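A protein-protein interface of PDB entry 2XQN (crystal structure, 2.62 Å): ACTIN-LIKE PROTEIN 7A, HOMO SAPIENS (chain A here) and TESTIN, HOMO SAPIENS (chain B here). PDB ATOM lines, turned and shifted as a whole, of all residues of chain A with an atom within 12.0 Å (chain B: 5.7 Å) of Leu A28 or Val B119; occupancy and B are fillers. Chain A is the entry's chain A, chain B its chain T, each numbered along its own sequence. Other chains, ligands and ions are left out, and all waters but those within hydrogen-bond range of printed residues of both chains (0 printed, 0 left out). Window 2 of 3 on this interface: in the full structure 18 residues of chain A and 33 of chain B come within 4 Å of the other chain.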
ATOM      1  N   LEU A  28       6.792  10.721  14.085  1.00  0.00           N
ATOM      2  CA  LEU A  28       6.333  10.592  15.508  1.00  0.00           C
ATOM      3  C   LEU A  28       7.088   9.537  16.434  1.00  0.00           C
ATOM      4  O   LEU A  28       7.709   8.550  15.958  1.00  0.00           O
ATOM      5  CB  LEU A  28       4.774  10.576  15.584  1.00  0.00           C
ATOM      6  CG  LEU A  28       3.881   9.684  14.698  1.00  0.00           C
ATOM      7  CD1 LEU A  28       3.583   8.419  15.437  1.00  0.00           C
ATOM      8  CD2 LEU A  28       2.562  10.330  14.307  1.00  0.00           C
ATOM      9  N   GLN A  29       7.027   9.796  17.751  1.00  0.00           N
ATOM     10  CA  GLN A  29       7.839   9.151  18.818  1.00  0.00           C
ATOM     11  C   GLN A  29       7.148   7.905  19.472  1.00  0.00           C
ATOM     12  O   GLN A  29       6.007   7.607  19.138  1.00  0.00           O
ATOM     13  CB  GLN A  29       8.131  10.222  19.889  1.00  0.00           C
ATOM     14  CG  GLN A  29       8.456  11.693  19.377  1.00  0.00           C
ATOM     15  CD  GLN A  29       7.278  12.451  18.742  1.00  0.00           C
ATOM     16  N   THR A  30       7.810   7.183  20.390  1.00  0.00           N
ATOM     17  CA  THR A  30       7.159   6.030  21.105  1.00  0.00           C
ATOM     18  C   THR A  30       7.020   6.150  22.651  1.00  0.00           C
ATOM     19  O   THR A  30       7.944   6.610  23.344  1.00  0.00           O
ATOM     20  CB  THR A  30       7.704   4.603  20.655  1.00  0.00           C
ATOM     21  OG1 THR A  30       7.310   4.354  19.305  1.00  0.00           O
ATOM     22  CG2 THR A  30       7.172   3.419  21.532  1.00  0.00           C
ATOM     23  N   ALA A  31       5.839   5.768  23.166  1.00  0.00           N
ATOM     24  CA  ALA A  31       5.569   5.765  24.627  1.00  0.00           C
ATOM     25  C   ALA A  31       6.344   4.680  25.393  1.00  0.00           C
ATOM     26  O   ALA A  31       6.161   3.470  25.162  1.00  0.00           O
ATOM     27  CB  ALA A  31       4.067   5.655  24.926  1.00  0.00           C
ATOM     28  N   SER A  32       7.198   5.139  26.311  1.00  0.00           N
ATOM     29  CA  SER A  32       8.065   4.250  27.067  1.00  0.00           C
ATOM     30  C   SER A  32       7.752   4.304  28.589  1.00  0.00           C
ATOM     31  O   SER A  32       7.976   5.325  29.248  1.00  0.00           O
ATOM     32  CB  SER A  32       9.531   4.607  26.743  1.00  0.00           C
ATOM     33  OG  SER A  32      10.412   3.576  27.157  1.00  0.00           O
ATOM     34  N   LYS B 107       2.964   4.809  19.111  1.00  0.00           N
ATOM     35  CA  LYS B 107       3.573   6.001  18.541  1.00  0.00           C
ATOM     36  C   LYS B 107       2.676   7.249  18.851  1.00  0.00           C
ATOM     37  O   LYS B 107       1.441   7.177  18.786  1.00  0.00           O
ATOM     38  CB  LYS B 107       3.785   5.779  17.023  1.00  0.00           C
ATOM     39  CG  LYS B 107       5.126   5.093  16.621  1.00  0.00           C
ATOM     40  CD  LYS B 107       5.092   4.439  15.220  1.00  0.00           C
ATOM     41  N   PHE B 108       3.281   8.378  19.205  1.00  0.00           N
ATOM     42  CA  PHE B 108       2.507   9.575  19.531  1.00  0.00           C
ATOM     43  C   PHE B 108       3.180  10.897  19.106  1.00  0.00           C
ATOM     44  O   PHE B 108       4.308  10.906  18.639  1.00  0.00           O
ATOM     45  CB  PHE B 108       2.235   9.608  21.029  1.00  0.00           C
ATOM     46  CG  PHE B 108       3.408  10.061  21.846  1.00  0.00           C
ATOM     47  CD1 PHE B 108       4.475   9.188  22.110  1.00  0.00           C
ATOM     48  CD2 PHE B 108       3.448  11.360  22.356  1.00  0.00           C
ATOM     49  CE1 PHE B 108       5.592   9.610  22.863  1.00  0.00           C
ATOM     50  CE2 PHE B 108       4.526  11.794  23.131  1.00  0.00           C
ATOM     51  CZ  PHE B 108       5.612  10.919  23.384  1.00  0.00           C
ATOM     52  N   MET B 109       2.499  12.018  19.294  1.00  0.00           N
ATOM     53  CA  MET B 109       3.061  13.312  18.979  1.00  0.00           C
ATOM     54  C   MET B 109       2.681  14.352  20.046  1.00  0.00           C
ATOM     55  O   MET B 109       1.513  14.729  20.156  1.00  0.00           O
ATOM     56  CB  MET B 109       2.523  13.733  17.642  1.00  0.00           C
ATOM     57  CG  MET B 109       3.015  15.080  17.150  1.00  0.00           C
ATOM     58  SD  MET B 109       2.348  15.395  15.499  1.00  0.00           S
ATOM     59  CE  MET B 109       2.879  13.886  14.617  1.00  0.00           C
ATOM     60  N   CYS B 117      -2.225  10.708  18.677  1.00  0.00           N
ATOM     61  CA  CYS B 117      -1.823   9.412  18.115  1.00  0.00           C
ATOM     62  C   CYS B 117      -1.155   9.510  16.731  1.00  0.00           C
ATOM     63  O   CYS B 117      -0.549   8.541  16.267  1.00  0.00           O
ATOM     64  CB  CYS B 117      -3.049   8.493  18.005  1.00  0.00           C
ATOM     65  SG  CYS B 117      -4.247   9.124  16.810  1.00  0.00           S
ATOM     66  N   SER B 118      -1.272  10.673  16.089  1.00  0.00           N
ATOM     67  CA  SER B 118      -1.050  10.824  14.661  1.00  0.00           C
ATOM     68  C   SER B 118      -0.936  12.310  14.258  1.00  0.00           C
ATOM     69  O   SER B 118      -1.409  13.197  14.996  1.00  0.00           O
ATOM     70  CB  SER B 118      -2.247  10.217  13.939  1.00  0.00           C
ATOM     71  OG  SER B 118      -3.370  11.072  14.068  1.00  0.00           O
ATOM     72  N   VAL B 119      -0.357  12.575  13.077  1.00  0.00           N
ATOM     73  CA  VAL B 119      -0.328  13.926  12.489  1.00  0.00           C
ATOM     74  C   VAL B 119      -1.751  14.488  12.220  1.00  0.00           C
ATOM     75  O   VAL B 119      -2.013  15.704  12.434  1.00  0.00           O
ATOM     76  CB  VAL B 119       0.551  14.001  11.156  1.00  0.00           C
ATOM     77  CG1 VAL B 119       0.699  15.492  10.654  1.00  0.00           C
ATOM     78  CG2 VAL B 119       1.960  13.321  11.323  1.00  0.00           C
ATOM     79  N   GLU B 120      -2.631  13.604  11.728  1.00  0.00           N
ATOM     80  CA  GLU B 120      -4.049  13.895  11.458  1.00  0.00           C
ATOM     81  C   GLU B 120      -4.644  14.575  12.671  1.00  0.00           C
ATOM     82  O   GLU B 120      -5.225  15.661  12.578  1.00  0.00           O
ATOM     83  CB  GLU B 120      -4.849  12.583  11.249  1.00  0.00           C
ATOM     84  CG  GLU B 120      -4.620  11.811   9.935  1.00  0.00           C
ATOM     85  CD  GLU B 120      -3.167  11.314   9.715  1.00  0.00           C
ATOM     86  OE1 GLU B 120      -2.270  11.535  10.569  1.00  0.00           O
ATOM     87  OE2 GLU B 120      -2.911  10.701   8.657  1.00  0.00           O
ATOM     88  N   CYS B 121      -4.475  13.899  13.815  1.00  0.00           N
ATOM     89  CA  CYS B 121      -5.130  14.255  15.061  1.00  0.00           C
ATOM     90  C   CYS B 121      -4.581  15.571  15.610  1.00  0.00           C
ATOM     91  O   CYS B 121      -5.361  16.411  16.076  1.00  0.00           O
ATOM     92  CB  CYS B 121      -4.994  13.108  16.070  1.00  0.00           C
ATOM     93  SG  CYS B 121      -6.205  11.725  15.889  1.00  0.00           S
ATOM     94  N   LYS B 122      -3.250  15.736  15.542  1.00  0.00           N
ATOM     95  CA  LYS B 122      -2.585  17.036  15.758  1.00  0.00           C
ATOM     96  C   LYS B 122      -3.084  18.108  14.801  1.00  0.00           C
ATOM     97  O   LYS B 122      -3.246  19.242  15.213  1.00  0.00           O
ATOM     98  CB  LYS B 122      -1.059  16.949  15.645  1.00  0.00           C
ATOM     99  CG  LYS B 122      -0.362  18.172  16.265  1.00  0.00           C
ATOM    100  CD  LYS B 122       0.496  18.951  15.266  1.00  0.00           C
ATOM    101  CE  LYS B 122       0.331  20.456  15.507  1.00  0.00           C
ATOM    102  NZ  LYS B 122       1.205  21.196  14.594  1.00  0.00           N
ATOM    103  N   LYS B 123      -3.338  17.728  13.539  1.00  0.00           N
ATOM    104  CA  LYS B 123      -3.857  18.660  12.503  1.00  0.00           C
ATOM    105  C   LYS B 123      -5.343  19.104  12.662  1.00  0.00           C
ATOM    106  O   LYS B 123      -5.642  20.265  12.389  1.00  0.00           O
ATOM    107  CB  LYS B 123      -3.447  18.270  11.055  1.00  0.00           C
ATOM    108  CG  LYS B 123      -2.071  18.840  10.586  1.00  0.00           C
ATOM    109  CD  LYS B 123      -1.727  18.481   9.111  1.00  0.00           C
ATOM    110  N   ARG B 124      -6.251  18.229  13.120  1.00  0.00           N
ATOM    111  CA  ARG B 124      -7.432  18.722  13.866  1.00  0.00           C
ATOM    112  C   ARG B 124      -6.900  19.407  15.107  1.00  0.00           C
ATOM    113  O   ARG B 124      -5.689  19.452  15.317  1.00  0.00           O
ATOM    114  CB  ARG B 124      -8.301  17.589  14.348  1.00  0.00           C
ATOM    115  CG  ARG B 124      -8.900  16.814  13.291  1.00  0.00           C
ATOM    116  CD  ARG B 124     -10.037  17.592  12.651  1.00  0.00           C
ATOM    117  NE  ARG B 124     -11.214  16.732  12.587  1.00  0.00           N
ATOM    118  CZ  ARG B 124     -11.286  15.589  11.898  1.00  0.00           C
ATOM    119  NH1 ARG B 124     -10.249  15.167  11.170  1.00  0.00           N
ATOM    120  NH2 ARG B 124     -12.409  14.872  11.936  1.00  0.00           N
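The backbone NH of Phe B108 is in hydrogen-bond range of the backbone carbonyl oxygen of Gln A29, at 2.8 Å.
Printed residues of chain B that touch a printed residue of chain A: Lys B107, Phe B108, Met B109, Ser B118 and Val B119. Of the 5 printed residues of chain A, 4 touch a printed residue of chain B. Hydrophobic or aromatic side chains of chain A that line the printed part of chain B: Leu A28.
The side-chain hydroxyl (OG) of Ser B118 sits at hydrogen-bond distance from the backbone NH (N) of Cys B121 (3.0 Å). SG of Cys B117 lies close to OG of Ser B118 (3.5 Å).
Among the printed residues, pairs that only touch across the chains: Leu A28 with Lys B107 (3.1 Å), Leu A28 with Phe B108 (3.1 Å), Leu A28 with Met B109 (3.6 Å), Leu A28 with Ser B118 (3.7 Å), Leu A28 with Val B119 (3.9 Å), Gln A29 with Lys B107 (3.0 Å), Thr A30 with Lys B107 (3.5 Å), Thr A30 with Phe B108 (3.7 Å) and Ala A31 with Phe B108 (3.8 Å).
Of chain B, only Lys B107, Phe B108, Met B109, Ser B118 and Val B119 come within 4 Å of Leu A28. Printed residues of chain B within 4 Å of Thr A30: Lys B107 and Phe B108. Printed residues of chain B within 4 Å of Ala A31: Phe B108. Ser A32 touches none of the printed residues of chain B. Lys B107 touches three residues of chain A. No residue of chain A comes within 4 Å of Cys B117. Of the printed residues of chain A, Ser B118 touches Leu A28. Glu B120 touches none of the printed residues of chain A. No residue of chain A comes within 4 Å of Cys B121. No residue of chain A comes within 4 Å of Lys B123. The nearest residue of chain A that does not touch Val B119 is Gln A29 (8.9 Å).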
